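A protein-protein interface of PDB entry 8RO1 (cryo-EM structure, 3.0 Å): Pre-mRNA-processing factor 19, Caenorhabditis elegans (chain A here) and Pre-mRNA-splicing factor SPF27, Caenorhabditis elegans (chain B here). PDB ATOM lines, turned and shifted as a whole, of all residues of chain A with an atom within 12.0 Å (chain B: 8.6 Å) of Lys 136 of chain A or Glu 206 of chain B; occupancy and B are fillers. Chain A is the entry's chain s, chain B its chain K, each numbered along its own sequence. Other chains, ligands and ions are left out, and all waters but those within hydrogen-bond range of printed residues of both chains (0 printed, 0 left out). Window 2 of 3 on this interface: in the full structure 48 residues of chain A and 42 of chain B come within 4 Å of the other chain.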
ATOM      1  N   ALA A 127       8.169  14.995   3.634  1.00  0.00           N
ATOM      2  CA  ALA A 127       8.186  14.742   5.070  1.00  0.00           C
ATOM      3  C   ALA A 127       9.456  15.271   5.715  1.00  0.00           C
ATOM      4  O   ALA A 127       9.417  15.783   6.838  1.00  0.00           O
ATOM      5  CB  ALA A 127       8.040  13.251   5.345  1.00  0.00           C
ATOM      6  N   ALA A 128      10.594  15.145   5.038  1.00  0.00           N
ATOM      7  CA  ALA A 128      11.826  15.692   5.588  1.00  0.00           C
ATOM      8  C   ALA A 128      11.781  17.213   5.642  1.00  0.00           C
ATOM      9  O   ALA A 128      12.146  17.814   6.658  1.00  0.00           O
ATOM     10  CB  ALA A 128      13.021  15.218   4.764  1.00  0.00           C
ATOM     11  N   ARG A 129      11.330  17.860   4.570  1.00  0.00           N
ATOM     12  CA  ARG A 129      11.216  19.314   4.601  1.00  0.00           C
ATOM     13  C   ARG A 129      10.135  19.802   5.551  1.00  0.00           C
ATOM     14  O   ARG A 129      10.231  20.919   6.064  1.00  0.00           O
ATOM     15  CB  ARG A 129      10.938  19.866   3.210  1.00  0.00           C
ATOM     16  CG  ARG A 129      12.129  19.826   2.304  1.00  0.00           C
ATOM     17  CD  ARG A 129      12.042  20.839   1.197  1.00  0.00           C
ATOM     18  NE  ARG A 129      13.324  20.884   0.511  1.00  0.00           N
ATOM     19  CZ  ARG A 129      13.902  21.968   0.010  1.00  0.00           C
ATOM     20  NH1 ARG A 129      15.145  21.875  -0.449  1.00  0.00           N
ATOM     21  NH2 ARG A 129      13.273  23.133  -0.070  1.00  0.00           N
ATOM     22  N   GLU A 130       9.091  19.013   5.777  1.00  0.00           N
ATOM     23  CA  GLU A 130       8.100  19.379   6.782  1.00  0.00           C
ATOM     24  C   GLU A 130       8.700  19.345   8.183  1.00  0.00           C
ATOM     25  O   GLU A 130       8.414  20.218   9.007  1.00  0.00           O
ATOM     26  CB  GLU A 130       6.896  18.443   6.671  1.00  0.00           C
ATOM     27  CG  GLU A 130       5.747  18.667   7.652  1.00  0.00           C
ATOM     28  CD  GLU A 130       4.861  19.825   7.242  1.00  0.00           C
ATOM     29  OE1 GLU A 130       5.371  20.791   6.640  1.00  0.00           O
ATOM     30  OE2 GLU A 130       3.644  19.765   7.513  1.00  0.00           O
ATOM     31  N   ALA A 131       9.524  18.338   8.471  1.00  0.00           N
ATOM     32  CA  ALA A 131      10.190  18.262   9.766  1.00  0.00           C
ATOM     33  C   ALA A 131      11.104  19.453  10.001  1.00  0.00           C
ATOM     34  O   ALA A 131      11.181  19.969  11.120  1.00  0.00           O
ATOM     35  CB  ALA A 131      10.982  16.963   9.875  1.00  0.00           C
ATOM     36  N   LEU A 132      11.806  19.906   8.965  1.00  0.00           N
ATOM     37  CA  LEU A 132      12.589  21.131   9.076  1.00  0.00           C
ATOM     38  C   LEU A 132      11.701  22.351   9.282  1.00  0.00           C
ATOM     39  O   LEU A 132      11.960  23.174  10.163  1.00  0.00           O
ATOM     40  CB  LEU A 132      13.452  21.311   7.833  1.00  0.00           C
ATOM     41  CG  LEU A 132      14.689  20.428   7.693  1.00  0.00           C
ATOM     42  CD1 LEU A 132      15.196  20.477   6.269  1.00  0.00           C
ATOM     43  CD2 LEU A 132      15.792  20.833   8.647  1.00  0.00           C
ATOM     44  N   SER A 133      10.644  22.483   8.482  1.00  0.00           N
ATOM     45  CA  SER A 133       9.794  23.669   8.538  1.00  0.00           C
ATOM     46  C   SER A 133       9.026  23.814   9.848  1.00  0.00           C
ATOM     47  O   SER A 133       8.531  24.908  10.125  1.00  0.00           O
ATOM     48  CB  SER A 133       8.813  23.656   7.374  1.00  0.00           C
ATOM     49  OG  SER A 133       9.503  23.692   6.138  1.00  0.00           O
ATOM     50  N   THR A 134       8.880  22.743  10.630  1.00  0.00           N
ATOM     51  CA  THR A 134       8.191  22.777  11.919  1.00  0.00           C
ATOM     52  C   THR A 134       9.112  22.379  13.066  1.00  0.00           C
ATOM     53  O   THR A 134       8.630  22.032  14.146  1.00  0.00           O
ATOM     54  CB  THR A 134       6.965  21.867  11.901  1.00  0.00           C
ATOM     55  OG1 THR A 134       7.371  20.517  11.652  1.00  0.00           O
ATOM     56  CG2 THR A 134       5.977  22.306  10.840  1.00  0.00           C
ATOM     57  N   LEU A 135      10.423  22.407  12.850  1.00  0.00           N
ATOM     58  CA  LEU A 135      11.373  21.917  13.838  1.00  0.00           C
ATOM     59  C   LEU A 135      11.319  22.795  15.085  1.00  0.00           C
ATOM     60  O   LEU A 135      11.577  24.000  15.013  1.00  0.00           O
ATOM     61  CB  LEU A 135      12.768  21.912  13.226  1.00  0.00           C
ATOM     62  CG  LEU A 135      13.948  21.407  14.032  1.00  0.00           C
ATOM     63  CD1 LEU A 135      13.762  19.950  14.370  1.00  0.00           C
ATOM     64  CD2 LEU A 135      15.204  21.595  13.209  1.00  0.00           C
ATOM     65  N   LYS A 136      10.947  22.194  16.220  1.00  0.00           N
ATOM     66  CA  LYS A 136      10.951  22.806  17.539  1.00  0.00           C
ATOM     67  C   LYS A 136      11.772  21.977  18.519  1.00  0.00           C
ATOM     68  O   LYS A 136      11.789  20.748  18.408  1.00  0.00           O
ATOM     69  CB  LYS A 136       9.535  22.928  18.090  1.00  0.00           C
ATOM     70  CG  LYS A 136       8.691  23.938  17.381  1.00  0.00           C
ATOM     71  CD  LYS A 136       7.361  24.090  18.075  1.00  0.00           C
ATOM     72  CE  LYS A 136       6.546  25.197  17.451  1.00  0.00           C
ATOM     73  NZ  LYS A 136       5.274  25.408  18.184  1.00  0.00           N
ATOM     74  N   PRO A 137      12.476  22.604  19.479  1.00  0.00           N
ATOM     75  CA  PRO A 137      13.243  21.747  20.386  1.00  0.00           C
ATOM     76  C   PRO A 137      12.337  20.937  21.312  1.00  0.00           C
ATOM     77  O   PRO A 137      12.815  20.336  22.274  1.00  0.00           O
ATOM     78  CB  PRO A 137      14.086  22.742  21.183  1.00  0.00           C
ATOM     79  CG  PRO A 137      13.327  23.992  21.132  1.00  0.00           C
ATOM     80  CD  PRO A 137      12.667  24.028  19.798  1.00  0.00           C
ATOM     81  N   VAL B 199      15.046  28.770   8.069  1.00  0.00           N
ATOM     82  CA  VAL B 199      14.770  27.587   8.881  1.00  0.00           C
ATOM     83  C   VAL B 199      15.749  27.504  10.043  1.00  0.00           C
ATOM     84  O   VAL B 199      15.363  27.245  11.187  1.00  0.00           O
ATOM     85  CB  VAL B 199      14.810  26.320   8.009  1.00  0.00           C
ATOM     86  CG1 VAL B 199      14.788  25.061   8.861  1.00  0.00           C
ATOM     87  CG2 VAL B 199      13.656  26.327   7.028  1.00  0.00           C
ATOM     88  N   THR B 200      17.036  27.696   9.756  1.00  0.00           N
ATOM     89  CA  THR B 200      18.044  27.686  10.811  1.00  0.00           C
ATOM     90  C   THR B 200      17.839  28.835  11.785  1.00  0.00           C
ATOM     91  O   THR B 200      18.036  28.676  12.993  1.00  0.00           O
ATOM     92  CB  THR B 200      19.444  27.795  10.210  1.00  0.00           C
ATOM     93  OG1 THR B 200      19.518  28.962   9.385  1.00  0.00           O
ATOM     94  CG2 THR B 200      19.772  26.590   9.351  1.00  0.00           C
ATOM     95  N   ASN B 201      17.455  30.004  11.277  1.00  0.00           N
ATOM     96  CA  ASN B 201      17.196  31.146  12.146  1.00  0.00           C
ATOM     97  C   ASN B 201      15.944  30.967  12.993  1.00  0.00           C
ATOM     98  O   ASN B 201      15.916  31.382  14.154  1.00  0.00           O
ATOM     99  CB  ASN B 201      17.077  32.399  11.293  1.00  0.00           C
ATOM    100  CG  ASN B 201      16.994  33.648  12.115  1.00  0.00           C
ATOM    101  OD1 ASN B 201      17.760  33.838  13.056  1.00  0.00           O
ATOM    102  ND2 ASN B 201      16.064  34.523  11.761  1.00  0.00           N
ATOM    103  N   ASN B 202      14.890  30.380  12.434  1.00  0.00           N
ATOM    104  CA  ASN B 202      13.656  30.205  13.194  1.00  0.00           C
ATOM    105  C   ASN B 202      13.823  29.202  14.320  1.00  0.00           C
ATOM    106  O   ASN B 202      13.309  29.410  15.420  1.00  0.00           O
ATOM    107  CB  ASN B 202      12.516  29.799  12.277  1.00  0.00           C
ATOM    108  CG  ASN B 202      11.888  30.982  11.585  1.00  0.00           C
ATOM    109  OD1 ASN B 202      10.906  31.537  12.062  1.00  0.00           O
ATOM    110  ND2 ASN B 202      12.455  31.383  10.471  1.00  0.00           N
ATOM    111  N   TYR B 203      14.516  28.097  14.064  1.00  0.00           N
ATOM    112  CA  TYR B 203      14.799  27.151  15.134  1.00  0.00           C
ATOM    113  C   TYR B 203      15.657  27.779  16.222  1.00  0.00           C
ATOM    114  O   TYR B 203      15.479  27.477  17.406  1.00  0.00           O
ATOM    115  CB  TYR B 203      15.504  25.919  14.587  1.00  0.00           C
ATOM    116  CG  TYR B 203      15.889  24.959  15.674  1.00  0.00           C
ATOM    117  CD1 TYR B 203      14.927  24.344  16.438  1.00  0.00           C
ATOM    118  CD2 TYR B 203      17.209  24.678  15.948  1.00  0.00           C
ATOM    119  CE1 TYR B 203      15.262  23.478  17.433  1.00  0.00           C
ATOM    120  CE2 TYR B 203      17.550  23.802  16.947  1.00  0.00           C
ATOM    121  CZ  TYR B 203      16.570  23.215  17.692  1.00  0.00           C
ATOM    122  OH  TYR B 203      16.889  22.325  18.687  1.00  0.00           O
ATOM    123  N   ARG B 204      16.611  28.632  15.840  1.00  0.00           N
ATOM    124  CA  ARG B 204      17.373  29.387  16.827  1.00  0.00           C
ATOM    125  C   ARG B 204      16.444  30.236  17.686  1.00  0.00           C
ATOM    126  O   ARG B 204      16.556  30.242  18.915  1.00  0.00           O
ATOM    127  CB  ARG B 204      18.413  30.244  16.096  1.00  0.00           C
ATOM    128  CG  ARG B 204      19.293  31.173  16.925  1.00  0.00           C
ATOM    129  CD  ARG B 204      20.157  30.443  17.931  1.00  0.00           C
ATOM    130  NE  ARG B 204      20.903  31.383  18.760  1.00  0.00           N
ATOM    131  CZ  ARG B 204      22.060  31.948  18.428  1.00  0.00           C
ATOM    132  NH1 ARG B 204      22.629  32.801  19.273  1.00  0.00           N
ATOM    133  NH2 ARG B 204      22.665  31.684  17.278  1.00  0.00           N
ATOM    134  N   MET B 205      15.488  30.927  17.061  1.00  0.00           N
ATOM    135  CA  MET B 205      14.524  31.719  17.819  1.00  0.00           C
ATOM    136  C   MET B 205      13.649  30.867  18.728  1.00  0.00           C
ATOM    137  O   MET B 205      13.229  31.337  19.788  1.00  0.00           O
ATOM    138  CB  MET B 205      13.641  32.547  16.893  1.00  0.00           C
ATOM    139  CG  MET B 205      14.378  33.666  16.221  1.00  0.00           C
ATOM    140  SD  MET B 205      13.329  34.802  15.325  1.00  0.00           S
ATOM    141  CE  MET B 205      12.749  33.789  13.986  1.00  0.00           C
ATOM    142  N   GLU B 206      13.344  29.630  18.336  1.00  0.00           N
ATOM    143  CA  GLU B 206      12.638  28.727  19.243  1.00  0.00           C
ATOM    144  C   GLU B 206      13.441  28.450  20.503  1.00  0.00           C
ATOM    145  O   GLU B 206      12.885  28.431  21.604  1.00  0.00           O
ATOM    146  CB  GLU B 206      12.324  27.409  18.544  1.00  0.00           C
ATOM    147  CG  GLU B 206      11.412  27.509  17.343  1.00  0.00           C
ATOM    148  CD  GLU B 206       9.949  27.521  17.709  1.00  0.00           C
ATOM    149  OE1 GLU B 206       9.625  27.663  18.907  1.00  0.00           O
ATOM    150  OE2 GLU B 206       9.117  27.382  16.790  1.00  0.00           O
ATOM    151  N   MET B 207      14.741  28.207  20.363  1.00  0.00           N
ATOM    152  CA  MET B 207      15.576  27.996  21.539  1.00  0.00           C
ATOM    153  C   MET B 207      15.702  29.268  22.366  1.00  0.00           C
ATOM    154  O   MET B 207      15.702  29.215  23.600  1.00  0.00           O
ATOM    155  CB  MET B 207      16.958  27.496  21.130  1.00  0.00           C
ATOM    156  CG  MET B 207      16.976  26.120  20.498  1.00  0.00           C
ATOM    157  SD  MET B 207      18.656  25.504  20.265  1.00  0.00           S
ATOM    158  CE  MET B 207      19.273  26.594  18.988  1.00  0.00           C
ATOM    159  N   GLU B 208      15.806  30.420  21.703  1.00  0.00           N
ATOM    160  CA  GLU B 208      15.915  31.689  22.413  1.00  0.00           C
ATOM    161  C   GLU B 208      14.658  32.002  23.212  1.00  0.00           C
ATOM    162  O   GLU B 208      14.750  32.429  24.367  1.00  0.00           O
ATOM    163  CB  GLU B 208      16.218  32.810  21.423  1.00  0.00           C
ATOM    164  CG  GLU B 208      17.613  32.723  20.807  1.00  0.00           C
ATOM    165  CD  GLU B 208      18.724  33.023  21.791  1.00  0.00           C
ATOM    166  OE1 GLU B 208      18.448  33.626  22.848  1.00  0.00           O
ATOM    167  OE2 GLU B 208      19.883  32.654  21.500  1.00  0.00           O
ATOM    168  N   ASN B 209      13.478  31.841  22.613  1.00  0.00           N
ATOM    169  CA  ASN B 209      12.248  32.139  23.345  1.00  0.00           C
ATOM    170  C   ASN B 209      12.085  31.228  24.552  1.00  0.00           C
ATOM    171  O   ASN B 209      11.630  31.672  25.610  1.00  0.00           O
ATOM    172  CB  ASN B 209      11.030  32.006  22.438  1.00  0.00           C
ATOM    173  CG  ASN B 209      10.970  33.076  21.387  1.00  0.00           C
ATOM    174  OD1 ASN B 209      11.655  34.086  21.470  1.00  0.00           O
ATOM    175  ND2 ASN B 209      10.169  32.846  20.365  1.00  0.00           N
ATOM    176  N   ARG B 210      12.415  29.946  24.411  1.00  0.00           N
ATOM    177  CA  ARG B 210      12.419  29.073  25.577  1.00  0.00           C
ATOM    178  C   ARG B 210      13.534  29.383  26.562  1.00  0.00           C
ATOM    179  O   ARG B 210      13.422  29.012  27.733  1.00  0.00           O
ATOM    180  CB  ARG B 210      12.552  27.625  25.131  1.00  0.00           C
ATOM    181  CG  ARG B 210      11.350  27.090  24.406  1.00  0.00           C
ATOM    182  CD  ARG B 210      11.627  25.687  23.915  1.00  0.00           C
ATOM    183  NE  ARG B 210      11.612  24.713  25.006  1.00  0.00           N
ATOM    184  CZ  ARG B 210      12.680  24.196  25.608  1.00  0.00           C
ATOM    185  NH1 ARG B 210      12.503  23.300  26.576  1.00  0.00           N
ATOM    186  NH2 ARG B 210      13.915  24.557  25.289  1.00  0.00           N
ATOM    187  N   GLN B 211      14.598  30.059  26.137  1.00  0.00           N
ATOM    188  CA  GLN B 211      15.617  30.478  27.091  1.00  0.00           C
ATOM    189  C   GLN B 211      15.140  31.669  27.906  1.00  0.00           C
ATOM    190  O   GLN B 211      15.373  31.730  29.116  1.00  0.00           O
ATOM    191  CB  GLN B 211      16.916  30.805  26.354  1.00  0.00           C
ATOM    192  CG  GLN B 211      18.069  31.237  27.244  1.00  0.00           C
ATOM    193  CD  GLN B 211      19.400  31.254  26.514  1.00  0.00           C
ATOM    194  OE1 GLN B 211      19.489  30.882  25.344  1.00  0.00           O
ATOM    195  NE2 GLN B 211      20.447  31.684  27.209  1.00  0.00           N
ATOM    196  N   ILE B 212      14.453  32.610  27.256  1.00  0.00           N
ATOM    197  CA  ILE B 212      13.910  33.776  27.943  1.00  0.00           C
ATOM    198  C   ILE B 212      12.785  33.395  28.892  1.00  0.00           C
ATOM    199  O   ILE B 212      12.475  34.162  29.807  1.00  0.00           O
ATOM    200  CB  ILE B 212      13.512  34.855  26.913  1.00  0.00           C
ATOM    201  CG1 ILE B 212      14.728  35.280  26.078  1.00  0.00           C
ATOM    202  CG2 ILE B 212      12.939  36.108  27.575  1.00  0.00           C
ATOM    203  CD1 ILE B 212      14.399  35.934  24.802  1.00  0.00           C
ATOM    204  N   ASP B 213      12.153  32.233  28.713  1.00  0.00           N
ATOM    205  CA  ASP B 213      11.262  31.670  29.733  1.00  0.00           C
ATOM    206  C   ASP B 213      11.925  31.446  31.097  1.00  0.00           C
ATOM    207  O   ASP B 213      11.222  31.084  32.046  1.00  0.00           O
ATOM    208  CB  ASP B 213      10.641  30.367  29.242  1.00  0.00           C
ATOM    209  CG  ASP B 213       9.492  30.594  28.274  1.00  0.00           C
ATOM    210  OD1 ASP B 213       8.857  31.670  28.310  1.00  0.00           O
ATOM    211  OD2 ASP B 213       9.215  29.688  27.465  1.00  0.00           O
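Of the printed residues of chain B, Leu 132 of chain A touches Val 199 (3.6 Å).
Of the printed residues of chain B, Leu 135 of chain A touches Tyr 203.
Of chain B, only Tyr 203, Glu 206 and Arg 210 come within 4 Å of Pro 137 of chain A.
Printed residues of chain A within 4 Å of Val 199 of chain B: Leu 132 (3.6 Å).
Asn 202 of chain B touches none of the printed residues of chain A.
Of the printed residues of chain A, Tyr 203 of chain B touches Leu 135, Lys 136 and Pro 137.
No residue of chain A comes within 4 Å of Met 205 of chain B.
Of the printed residues of chain A, Glu 206 of chain B touches Lys 136 (3.4 Å) and Pro 137 (3.6 Å).
No residue of chain A comes within 4 Å of Met 207 of chain B.
No residue of chain A comes within 4 Å of Glu 208 of chain B.
Printed residues of chain A within 4 Å of Arg 210 of chain B: Pro 137.
The nearest residue of chain A that does not touch Glu 206 of chain B is Leu 135 of chain A (4.2 Å).
Among the printed residues, merely in contact across the chains: Lys 136 of chain A with Glu 206 of chain B, Pro 137 of chain A with Tyr 203 of chain B, Pro 137 of chain A with Glu 206 of chain B, Leu 132 of chain A with Val 199 of chain B, Leu 135 of chain A with Tyr 203 of chain B, Pro 137 of chain A with Arg 210 of chain B and Lys 136 of chain A with Tyr 203 of chain B.
Hydrophobic or aromatic side chains of chain B within 4 Å of the printed part of chain A: Val 199 and Tyr 203.
Printed residues of chain A that touch a printed residue of chain B: Leu 132, Leu 135, Lys 136 and Pro 137.
Hydrophobic or aromatic side chains of chain A within 4 Å of the printed part of chain B: Leu 135 and Pro 137.
Among the printed residues, 7 pairs touch across the chains.
Among the printed residues, no Asp or Glu carboxylate lies within 4 Å of a Lys or Arg side-chain nitrogen of the other chain.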
